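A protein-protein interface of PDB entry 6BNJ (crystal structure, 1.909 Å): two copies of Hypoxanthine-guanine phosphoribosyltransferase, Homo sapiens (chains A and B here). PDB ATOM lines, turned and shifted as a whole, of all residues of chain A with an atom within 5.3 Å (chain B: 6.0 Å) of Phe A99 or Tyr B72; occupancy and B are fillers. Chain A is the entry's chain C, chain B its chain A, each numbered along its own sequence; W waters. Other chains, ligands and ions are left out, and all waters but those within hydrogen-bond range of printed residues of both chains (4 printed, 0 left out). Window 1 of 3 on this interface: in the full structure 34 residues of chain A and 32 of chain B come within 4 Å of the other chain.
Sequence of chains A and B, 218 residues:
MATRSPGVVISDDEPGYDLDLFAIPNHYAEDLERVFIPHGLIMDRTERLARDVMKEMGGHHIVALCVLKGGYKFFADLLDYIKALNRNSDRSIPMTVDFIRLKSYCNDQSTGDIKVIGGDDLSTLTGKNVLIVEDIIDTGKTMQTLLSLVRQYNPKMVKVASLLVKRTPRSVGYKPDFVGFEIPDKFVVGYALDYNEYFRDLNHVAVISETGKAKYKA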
ATOM      1  N   LEU A  65      33.230   2.941   6.241  1.00  0.00           N
ATOM      2  CA  LEU A  65      34.026   1.976   5.477  1.00  0.00           C
ATOM      3  C   LEU A  65      33.892   0.592   6.076  1.00  0.00           C
ATOM      4  O   LEU A  65      34.297   0.339   7.195  1.00  0.00           O
ATOM      5  CB  LEU A  65      35.510   2.367   5.450  1.00  0.00           C
ATOM      6  CG  LEU A  65      35.898   3.752   4.958  1.00  0.00           C
ATOM      7  CD1 LEU A  65      37.434   3.880   5.082  1.00  0.00           C
ATOM      8  CD2 LEU A  65      35.477   3.880   3.523  1.00  0.00           C
ATOM      9  N   CYS A  66      33.294  -0.301   5.324  1.00  0.00           N
ATOM     10  CA  CYS A  66      33.131  -1.697   5.772  1.00  0.00           C
ATOM     11  C   CYS A  66      34.372  -2.519   5.436  1.00  0.00           C
ATOM     12  O   CYS A  66      34.741  -2.585   4.283  1.00  0.00           O
ATOM     13  CB  CYS A  66      31.930  -2.300   5.077  1.00  0.00           C
ATOM     14  SG  CYS A  66      31.679  -4.031   5.424  1.00  0.00           S
ATOM     15  N   LEU A  68      35.497  -5.832   4.559  1.00  0.00           N
ATOM     16  CA  LEU A  68      35.093  -7.172   4.097  1.00  0.00           C
ATOM     17  C   LEU A  68      36.065  -8.272   4.496  1.00  0.00           C
ATOM     18  O   LEU A  68      37.240  -7.983   4.729  1.00  0.00           O
ATOM     19  CB  LEU A  68      34.953  -7.174   2.565  1.00  0.00           C
ATOM     20  CG  LEU A  68      33.954  -6.115   2.073  1.00  0.00           C
ATOM     21  CD1 LEU A  68      33.969  -5.958   0.529  1.00  0.00           C
ATOM     22  CD2 LEU A  68      32.556  -6.438   2.590  1.00  0.00           C
ATOM     23  N   PHE A  75      28.315  -4.103   9.919  1.00  0.00           N
ATOM     24  CA  PHE A  75      28.196  -2.873   9.147  1.00  0.00           C
ATOM     25  C   PHE A  75      26.736  -2.608   8.782  1.00  0.00           C
ATOM     26  O   PHE A  75      26.232  -1.510   9.028  1.00  0.00           O
ATOM     27  CB  PHE A  75      29.073  -2.980   7.882  1.00  0.00           C
ATOM     28  CG  PHE A  75      29.091  -1.754   7.018  1.00  0.00           C
ATOM     29  CD1 PHE A  75      29.920  -0.677   7.328  1.00  0.00           C
ATOM     30  CD2 PHE A  75      28.344  -1.704   5.846  1.00  0.00           C
ATOM     31  CE1 PHE A  75      29.995   0.438   6.475  1.00  0.00           C
ATOM     32  CE2 PHE A  75      28.409  -0.596   5.012  1.00  0.00           C
ATOM     33  CZ  PHE A  75      29.262   0.481   5.346  1.00  0.00           C
ATOM     34  N   ALA A  76      26.048  -3.604   8.233  1.00  0.00           N
ATOM     35  CA  ALA A  76      24.692  -3.358   7.722  1.00  0.00           C
ATOM     36  C   ALA A  76      23.762  -3.018   8.908  1.00  0.00           C
ATOM     37  O   ALA A  76      22.970  -2.063   8.821  1.00  0.00           O
ATOM     38  CB  ALA A  76      24.173  -4.577   6.922  1.00  0.00           C
ATOM     39  N   LEU A  79      24.616   0.448  10.564  1.00  0.00           N
ATOM     40  CA  LEU A  79      24.119   1.527   9.738  1.00  0.00           C
ATOM     41  C   LEU A  79      22.571   1.575   9.725  1.00  0.00           C
ATOM     42  O   LEU A  79      21.991   2.673   9.664  1.00  0.00           O
ATOM     43  CB  LEU A  79      24.674   1.412   8.328  1.00  0.00           C
ATOM     44  CG  LEU A  79      25.993   2.196   8.108  1.00  0.00           C
ATOM     45  CD1 LEU A  79      27.097   1.776   9.115  1.00  0.00           C
ATOM     46  CD2 LEU A  79      26.475   2.033   6.644  1.00  0.00           C
ATOM     47  N   LYS A  83      20.535   4.855  10.653  1.00  0.00           N
ATOM     48  CA  LYS A  83      19.447   5.382   9.819  1.00  0.00           C
ATOM     49  C   LYS A  83      18.154   5.582  10.643  1.00  0.00           C
ATOM     50  O   LYS A  83      17.441   6.546  10.458  1.00  0.00           O
ATOM     51  CB  LYS A  83      19.169   4.446   8.626  1.00  0.00           C
ATOM     52  CG  LYS A  83      19.989   4.758   7.409  1.00  0.00           C
ATOM     53  CD  LYS A  83      20.467   3.580   6.657  1.00  0.00           C
ATOM     54  CE  LYS A  83      19.347   2.839   6.069  1.00  0.00           C
ATOM     55  NZ  LYS A  83      19.843   1.443   5.897  1.00  0.00           N
ATOM     56  N   VAL A  97      29.016   5.353   1.838  1.00  0.00           N
ATOM     57  CA  VAL A  97      29.587   4.094   2.244  1.00  0.00           C
ATOM     58  C   VAL A  97      30.636   3.616   1.233  1.00  0.00           C
ATOM     59  O   VAL A  97      30.606   3.975   0.044  1.00  0.00           O
ATOM     60  CB  VAL A  97      28.493   2.997   2.430  1.00  0.00           C
ATOM     61  CG1 VAL A  97      27.455   3.423   3.504  1.00  0.00           C
ATOM     62  CG2 VAL A  97      27.803   2.653   1.085  1.00  0.00           C
ATOM     63  N   ASP A  98      31.568   2.805   1.719  1.00  0.00           N
ATOM     64  CA  ASP A  98      32.498   2.122   0.832  1.00  0.00           C
ATOM     65  C   ASP A  98      32.893   0.774   1.464  1.00  0.00           C
ATOM     66  O   ASP A  98      32.607   0.518   2.640  1.00  0.00           O
ATOM     67  CB  ASP A  98      33.709   3.008   0.564  1.00  0.00           C
ATOM     68  CG  ASP A  98      34.517   2.568  -0.680  1.00  0.00           C
ATOM     69  OD1 ASP A  98      34.072   1.669  -1.472  1.00  0.00           O
ATOM     70  OD2 ASP A  98      35.598   3.161  -0.865  1.00  0.00           O
ATOM     71  N   PHE A  99      33.505  -0.092   0.666  1.00  0.00           N
ATOM     72  CA  PHE A  99      33.810  -1.461   1.066  1.00  0.00           C
ATOM     73  C   PHE A  99      35.265  -1.757   0.675  1.00  0.00           C
ATOM     74  O   PHE A  99      35.699  -1.499  -0.464  1.00  0.00           O
ATOM     75  CB  PHE A  99      32.852  -2.467   0.411  1.00  0.00           C
ATOM     76  CG  PHE A  99      31.400  -2.149   0.650  1.00  0.00           C
ATOM     77  CD1 PHE A  99      30.750  -1.205  -0.140  1.00  0.00           C
ATOM     78  CD2 PHE A  99      30.693  -2.775   1.674  1.00  0.00           C
ATOM     79  CE1 PHE A  99      29.394  -0.877   0.107  1.00  0.00           C
ATOM     80  CE2 PHE A  99      29.364  -2.467   1.912  1.00  0.00           C
ATOM     81  CZ  PHE A  99      28.705  -1.527   1.119  1.00  0.00           C
ATOM     82  N   ILE A 100      36.038  -2.275   1.610  1.00  0.00           N
ATOM     83  CA  ILE A 100      37.423  -2.628   1.278  1.00  0.00           C
ATOM     84  C   ILE A 100      37.764  -3.969   1.839  1.00  0.00           C
ATOM     85  O   ILE A 100      37.202  -4.403   2.853  1.00  0.00           O
ATOM     86  CB  ILE A 100      38.433  -1.615   1.835  1.00  0.00           C
ATOM     87  CG1 ILE A 100      38.215  -1.490   3.339  1.00  0.00           C
ATOM     88  CG2 ILE A 100      38.222  -0.248   1.189  1.00  0.00           C
ATOM     89  CD1 ILE A 100      39.184  -0.590   4.052  1.00  0.00           C
ATOM     90  N   ARG A 101      38.675  -4.634   1.136  1.00  0.00           N
ATOM     91  CA  ARG A 101      39.302  -5.826   1.642  1.00  0.00           C
ATOM     92  C   ARG A 101      40.766  -5.528   2.020  1.00  0.00           C
ATOM     93  O   ARG A 101      41.379  -4.633   1.452  1.00  0.00           O
ATOM     94  CB  ARG A 101      39.238  -6.928   0.592  1.00  0.00           C
ATOM     95  CG  ARG A 101      37.836  -7.201   0.049  1.00  0.00           C
ATOM     96  CD  ARG A 101      37.855  -8.527  -0.663  1.00  0.00           C
ATOM     97  NE  ARG A 101      36.663  -8.760  -1.447  1.00  0.00           N
ATOM     98  CZ  ARG A 101      36.203  -9.970  -1.720  1.00  0.00           C
ATOM     99  NH1 ARG A 101      36.843 -11.041  -1.263  1.00  0.00           N
ATOM    100  NH2 ARG A 101      35.115 -10.103  -2.453  1.00  0.00           N
ATOM    101  N   ILE A 117      42.147  -3.267  -0.990  1.00  0.00           N
ATOM    102  CA  ILE A 117      41.533  -3.778  -2.216  1.00  0.00           C
ATOM    103  C   ILE A 117      40.061  -3.377  -2.353  1.00  0.00           C
ATOM    104  O   ILE A 117      39.291  -3.581  -1.404  1.00  0.00           O
ATOM    105  CB  ILE A 117      41.629  -5.313  -2.254  1.00  0.00           C
ATOM    106  CG1 ILE A 117      43.014  -5.767  -1.792  1.00  0.00           C
ATOM    107  CG2 ILE A 117      41.288  -5.859  -3.641  1.00  0.00           C
ATOM    108  CD1 ILE A 117      43.090  -7.240  -1.535  1.00  0.00           C
ATOM    109  N   GLY A 118      39.669  -2.794  -3.497  1.00  0.00           N
ATOM    110  CA  GLY A 118      38.250  -2.677  -3.886  1.00  0.00           C
ATOM    111  C   GLY A 118      37.345  -1.499  -3.477  1.00  0.00           C
ATOM    112  O   GLY A 118      36.089  -1.559  -3.620  1.00  0.00           O
ATOM    113  N   GLY A 119      37.959  -0.440  -2.956  1.00  0.00           N
ATOM    114  CA  GLY A 119      37.233   0.741  -2.541  1.00  0.00           C
ATOM    115  C   GLY A 119      37.384   1.869  -3.555  1.00  0.00           C
ATOM    116  O   GLY A 119      38.049   1.697  -4.590  1.00  0.00           O
ATOM    117  N   CYS B  66      27.498 -10.797  -3.865  1.00  0.00           N
ATOM    118  CA  CYS B  66      26.951  -9.437  -3.776  1.00  0.00           C
ATOM    119  C   CYS B  66      27.630  -8.532  -4.770  1.00  0.00           C
ATOM    120  O   CYS B  66      28.866  -8.384  -4.727  1.00  0.00           O
ATOM    121  CB  CYS B  66      27.140  -8.883  -2.370  1.00  0.00           C
ATOM    122  SG  CYS B  66      26.580  -7.210  -2.188  1.00  0.00           S
ATOM    123  N   VAL B  67      26.863  -7.932  -5.671  1.00  0.00           N
ATOM    124  CA  VAL B  67      27.429  -6.900  -6.547  1.00  0.00           C
ATOM    125  C   VAL B  67      27.407  -5.491  -5.893  1.00  0.00           C
ATOM    126  O   VAL B  67      26.360  -4.811  -5.763  1.00  0.00           O
ATOM    127  CB  VAL B  67      26.717  -6.888  -7.916  1.00  0.00           C
ATOM    128  CG1 VAL B  67      27.463  -5.945  -8.905  1.00  0.00           C
ATOM    129  CG2 VAL B  67      26.607  -8.338  -8.469  1.00  0.00           C
ATOM    130  N   LEU B  68      28.585  -5.072  -5.451  1.00  0.00           N
ATOM    131  CA  LEU B  68      28.766  -3.771  -4.752  1.00  0.00           C
ATOM    132  C   LEU B  68      28.756  -2.609  -5.729  1.00  0.00           C
ATOM    133  O   LEU B  68      29.113  -2.807  -6.891  1.00  0.00           O
ATOM    134  CB  LEU B  68      30.091  -3.777  -3.964  1.00  0.00           C
ATOM    135  CG  LEU B  68      30.125  -4.750  -2.782  1.00  0.00           C
ATOM    136  CD1 LEU B  68      31.512  -4.907  -2.228  1.00  0.00           C
ATOM    137  CD2 LEU B  68      29.091  -4.337  -1.697  1.00  0.00           C
ATOM    138  N   LYS B  69      28.405  -1.396  -5.274  1.00  0.00           N
ATOM    139  CA  LYS B  69      27.980  -1.135  -3.896  1.00  0.00           C
ATOM    140  C   LYS B  69      26.494  -1.338  -3.717  1.00  0.00           C
ATOM    141  O   LYS B  69      26.006  -1.670  -2.638  1.00  0.00           O
ATOM    142  CB  LYS B  69      28.303   0.309  -3.484  1.00  0.00           C
ATOM    143  CG  LYS B  69      29.775   0.639  -3.388  1.00  0.00           C
ATOM    144  CD  LYS B  69      29.903   2.136  -2.995  1.00  0.00           C
ATOM    145  CE  LYS B  69      31.322   2.651  -2.975  1.00  0.00           C
ATOM    146  NZ  LYS B  69      31.262   4.124  -2.707  1.00  0.00           N
ATOM    147  N   GLY B  70      25.775  -1.047  -4.786  1.00  0.00           N
ATOM    148  CA  GLY B  70      24.343  -0.973  -4.754  1.00  0.00           C
ATOM    149  C   GLY B  70      23.619  -2.231  -4.307  1.00  0.00           C
ATOM    150  O   GLY B  70      22.530  -2.128  -3.807  1.00  0.00           O
ATOM    151  N   GLY B  71      24.165  -3.418  -4.529  1.00  0.00           N
ATOM    152  CA  GLY B  71      23.426  -4.616  -4.073  1.00  0.00           C
ATOM    153  C   GLY B  71      23.522  -4.896  -2.577  1.00  0.00           C
ATOM    154  O   GLY B  71      22.877  -5.850  -2.082  1.00  0.00           O
ATOM    155  N   TYR B  72      24.302  -4.099  -1.839  1.00  0.00           N
ATOM    156  CA  TYR B  72      24.665  -4.518  -0.478  1.00  0.00           C
ATOM    157  C   TYR B  72      23.434  -4.617   0.487  1.00  0.00           C
ATOM    158  O   TYR B  72      23.416  -5.530   1.292  1.00  0.00           O
ATOM    159  CB  TYR B  72      25.773  -3.599   0.113  1.00  0.00           C
ATOM    160  CG  TYR B  72      25.321  -2.616   1.209  1.00  0.00           C
ATOM    161  CD1 TYR B  72      25.216  -3.035   2.536  1.00  0.00           C
ATOM    162  CD2 TYR B  72      25.038  -1.282   0.915  1.00  0.00           C
ATOM    163  CE1 TYR B  72      24.816  -2.158   3.548  1.00  0.00           C
ATOM    164  CE2 TYR B  72      24.632  -0.375   1.930  1.00  0.00           C
ATOM    165  CZ  TYR B  72      24.501  -0.830   3.242  1.00  0.00           C
ATOM    166  OH  TYR B  72      24.110   0.040   4.294  1.00  0.00           O
ATOM    167  N   LYS B  73      22.441  -3.699   0.412  1.00  0.00           N
ATOM    168  CA  LYS B  73      21.272  -3.771   1.329  1.00  0.00           C
ATOM    169  C   LYS B  73      20.354  -4.942   0.996  1.00  0.00           C
ATOM    170  O   LYS B  73      19.993  -5.730   1.865  1.00  0.00           O
ATOM    171  CB  LYS B  73      20.414  -2.486   1.291  1.00  0.00           C
ATOM    172  CG  LYS B  73      20.925  -1.397   2.121  1.00  0.00           C
ATOM    173  CD  LYS B  73      20.867  -1.750   3.605  1.00  0.00           C
ATOM    174  CE  LYS B  73      19.462  -2.023   4.051  1.00  0.00           C
ATOM    175  NZ  LYS B  73      19.431  -2.715   5.389  1.00  0.00           N
ATOM    176  N   PHE B  74      19.995  -5.049  -0.275  1.00  0.00           N
ATOM    177  CA  PHE B  74      19.233  -6.188  -0.774  1.00  0.00           C
ATOM    178  C   PHE B  74      19.909  -7.529  -0.404  1.00  0.00           C
ATOM    179  O   PHE B  74      19.240  -8.454   0.039  1.00  0.00           O
ATOM    180  CB  PHE B  74      19.062  -6.087  -2.284  1.00  0.00           C
ATOM    181  CG  PHE B  74      18.156  -7.168  -2.872  1.00  0.00           C
ATOM    182  CD1 PHE B  74      16.949  -7.496  -2.259  1.00  0.00           C
ATOM    183  CD2 PHE B  74      18.508  -7.815  -4.046  1.00  0.00           C
ATOM    184  CE1 PHE B  74      16.121  -8.474  -2.790  1.00  0.00           C
ATOM    185  CE2 PHE B  74      17.681  -8.782  -4.616  1.00  0.00           C
ATOM    186  CZ  PHE B  74      16.469  -9.103  -3.981  1.00  0.00           C
ATOM    187  N   PHE B  75      21.231  -7.609  -0.604  1.00  0.00           N
ATOM    188  CA  PHE B  75      22.008  -8.796  -0.285  1.00  0.00           C
ATOM    189  C   PHE B  75      21.887  -9.171   1.209  1.00  0.00           C
ATOM    190  O   PHE B  75      21.586 -10.317   1.558  1.00  0.00           O
ATOM    191  CB  PHE B  75      23.478  -8.515  -0.643  1.00  0.00           C
ATOM    192  CG  PHE B  75      24.436  -9.635  -0.310  1.00  0.00           C
ATOM    193  CD1 PHE B  75      24.572 -10.722  -1.184  1.00  0.00           C
ATOM    194  CD2 PHE B  75      25.249  -9.557   0.807  1.00  0.00           C
ATOM    195  CE1 PHE B  75      25.509 -11.755  -0.937  1.00  0.00           C
ATOM    196  CE2 PHE B  75      26.198 -10.576   1.070  1.00  0.00           C
ATOM    197  CZ  PHE B  75      26.323 -11.682   0.204  1.00  0.00           C
ATOM    198  N   ALA B  76      22.153  -8.190   2.063  1.00  0.00           N
ATOM    199  CA  ALA B  76      22.133  -8.425   3.510  1.00  0.00           C
ATOM    200  C   ALA B  76      20.715  -8.896   3.950  1.00  0.00           C
ATOM    201  O   ALA B  76      20.585  -9.887   4.684  1.00  0.00           O
ATOM    202  CB  ALA B  76      22.556  -7.156   4.277  1.00  0.00           C
ATOM    203  N   ASP B  77      19.683  -8.204   3.486  1.00  0.00           N
ATOM    204  CA  ASP B  77      18.299  -8.559   3.868  1.00  0.00           C
ATOM    205  C   ASP B  77      17.857  -9.899   3.261  1.00  0.00           C
ATOM    206  O   ASP B  77      17.213 -10.721   3.931  1.00  0.00           O
ATOM    207  CB  ASP B  77      17.309  -7.439   3.470  1.00  0.00           C
ATOM    208  CG  ASP B  77      17.514  -6.171   4.288  1.00  0.00           C
ATOM    209  OD1 ASP B  77      18.060  -6.286   5.415  1.00  0.00           O
ATOM    210  OD2 ASP B  77      17.119  -5.062   3.830  1.00  0.00           O
ATOM    211  N   PHE B  99      32.006 -10.984  -2.602  1.00  0.00           N
ATOM    212  CA  PHE B  99      31.640  -9.653  -3.043  1.00  0.00           C
ATOM    213  C   PHE B  99      32.410  -9.359  -4.303  1.00  0.00           C
ATOM    214  O   PHE B  99      33.535  -9.826  -4.474  1.00  0.00           O
ATOM    215  CB  PHE B  99      31.928  -8.597  -1.944  1.00  0.00           C
ATOM    216  CG  PHE B  99      31.209  -8.877  -0.668  1.00  0.00           C
ATOM    217  CD1 PHE B  99      31.700  -9.816   0.235  1.00  0.00           C
ATOM    218  CD2 PHE B  99      29.992  -8.230  -0.386  1.00  0.00           C
ATOM    219  CE1 PHE B  99      31.027 -10.093   1.426  1.00  0.00           C
ATOM    220  CE2 PHE B  99      29.304  -8.503   0.787  1.00  0.00           C
ATOM    221  CZ  PHE B  99      29.805  -9.435   1.695  1.00  0.00           C
ATOM    222  N   ARG B 101      32.889  -5.935  -7.261  1.00  0.00           N
ATOM    223  CA  ARG B 101      32.469  -4.576  -7.542  1.00  0.00           C
ATOM    224  C   ARG B 101      32.646  -4.312  -9.001  1.00  0.00           C
ATOM    225  O   ARG B 101      33.671  -4.692  -9.570  1.00  0.00           O
ATOM    226  CB  ARG B 101      33.261  -3.568  -6.720  1.00  0.00           C
ATOM    227  CG  ARG B 101      33.131  -2.164  -7.283  1.00  0.00           C
ATOM    228  CD  ARG B 101      32.442  -1.244  -6.317  1.00  0.00           C
ATOM    229  NE  ARG B 101      33.383  -0.526  -5.480  1.00  0.00           N
ATOM    230  CZ  ARG B 101      33.629   0.779  -5.564  1.00  0.00           C
ATOM    231  NH1 ARG B 101      32.996   1.548  -6.446  1.00  0.00           N
ATOM    232  NH2 ARG B 101      34.509   1.318  -4.737  1.00  0.00           N
ATOM    233  N   ALA B 192      20.235   1.655  -0.859  1.00  0.00           N
ATOM    234  CA  ALA B 192      21.598   1.524  -1.393  1.00  0.00           C
ATOM    235  C   ALA B 192      21.788   1.965  -2.857  1.00  0.00           C
ATOM    236  O   ALA B 192      22.924   1.978  -3.332  1.00  0.00           O
ATOM    237  CB  ALA B 192      22.097   0.108  -1.250  1.00  0.00           C
ATOM    238  N   ARG B 200      22.314   6.392  -0.435  1.00  0.00           N
ATOM    239  CA  ARG B 200      22.434   5.014  -0.017  1.00  0.00           C
ATOM    240  C   ARG B 200      21.958   4.850   1.423  1.00  0.00           C
ATOM    241  O   ARG B 200      21.493   3.766   1.795  1.00  0.00           O
ATOM    242  CB  ARG B 200      23.884   4.483  -0.160  1.00  0.00           C
ATOM    243  CG  ARG B 200      24.403   4.553  -1.582  1.00  0.00           C
ATOM    244  CD  ARG B 200      25.584   3.568  -1.770  1.00  0.00           C
ATOM    245  NE  ARG B 200      26.439   3.924  -2.891  1.00  0.00           N
ATOM    246  CZ  ARG B 200      26.330   3.431  -4.109  1.00  0.00           C
ATOM    247  NH1 ARG B 200      25.361   2.544  -4.378  1.00  0.00           N
ATOM    248  NH2 ARG B 200      27.197   3.822  -5.057  1.00  0.00           N
HETATM  249  O   HOH W   1      20.362   1.631   2.927  1.00  0.00           O
HETATM  250  O   HOH W   2      27.808   5.886  -0.840  1.00  0.00           O
HETATM  251  O   HOH W   3      22.758   2.500   4.631  1.00  0.00           O
HETATM  252  O   HOH W   4      22.508  -1.005   6.342  1.00  0.00           O
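NZ of Lys B69 sits at hydrogen-bond distance from O of Val A97, 2.8 Å away. The side-chain amino group of Lys B69 is in salt-bridge range of the side-chain carboxylate of Asp A98 (3.9 Å). O of Phe B99 is in hydrogen-bond range of NH2 of Arg A101, 2.6 Å away. The side-chain carboxylate (OD1) of Asp A98 lies within salt-bridge range of the guanidinium group (NH2) of Arg B101 (3.3 Å). NE of Arg B101 sits at hydrogen-bond distance from O of Gly A118.
The side-chain carboxylate of Asp B77 lies within salt-bridge range of the side-chain amino group of Lys B73 (3.6 Å). The backbone carbonyl oxygen (O) of Ala B192 sits at hydrogen-bond distance from the guanidinium group (NH1) of Arg B200, at 2.7 Å. The backbone NH (N) of Cys A66 lies within hydrogen-bond range of the backbone carbonyl oxygen (O) of Asp A98 (2.9 Å). N of Leu A68 lies within hydrogen-bond range of O of Ile A100 (2.8 Å). The backbone NH (N) of Arg A101 lies within hydrogen-bond range of the backbone carbonyl oxygen (O) of Ile A117, 2.8 Å away.
Leu A68 touches Leu B68. Leu A79 touches Tyr B72 (CD2 to OH, 3.9 Å). Lys B73 touches Lys A83. CG2 of Val A97 touches CD of Arg B200, 3.7 Å away. Leu B68 touches Phe A99. Lys B69 touches Phe A99. CG of Tyr B72 touches CZ of Phe A99, at 3.6 Å. NH2 of Arg B101 touches C of Gly A119, 3.2 Å away.
Leu A65 touches none of the printed residues of chain B. Of the printed residues of chain B, Leu A79 touches Tyr B72 (3.9 Å). Of chain B, only Leu B68 (3.8 Å), Lys B69 (3.8 Å) and Tyr B72 (3.6 Å) come within 4 Å of Phe A99. Of the printed residues of chain A, Lys B69 touches Val A97, Asp A98 and Phe A99. Of chain A, only Leu A79 and Phe A99 come within 4 Å of Tyr B72. Printed residues of chain A within 4 Å of Lys B73: Lys A83 (3.9 Å). The nearest printed residue of chain A that does not touch Tyr B72 is Phe A75 (4.2 Å).
Hydrophobic or aromatic side chains of chain B that line the printed part of chain A: Leu B68, Tyr B72 and Phe B99. Hydrophobic or aromatic side chains of chain A within 4 Å of the printed part of chain B: Leu A68, Leu A79, Val A97 and Phe A99. Among the printed residues, Asp or Glu carboxylates within 4 Å of a Lys or Arg side-chain nitrogen of the other chain: Asp A98 with Lys B69 and Asp A98 with Arg B101.
Leu A68 touches its own counterpart, Leu B68. Phe A99 touches Leu B68, but with the chains exchanged Leu A68 does not touch Phe B99 (4.1 Å). Arg A101 touches Phe B99, but with the chains exchanged Phe A99 does not touch Arg B101 (5.3 Å). Positions printed for both chains: 66, 68, 75, 76, 99 and 101.
Water W1 bridges O of Arg B200 (2.7 Å) and NZ of Lys A83 (3.0 Å). Water W4 bridges O of Ala A76 (2.7 Å) and OH of Tyr B72 (2.8 Å). Water W3 lies within hydrogen-bond range of OH of Tyr B72 (2.8 Å), NZ of Lys A83 (3.3 Å) and O of Arg B200 (3.4 Å). Water W2 lies within hydrogen-bond range of the backbone NH (N) of Val A97 (3.0 Å) and the guanidinium group (NE) of Arg B200 (3.2 Å).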
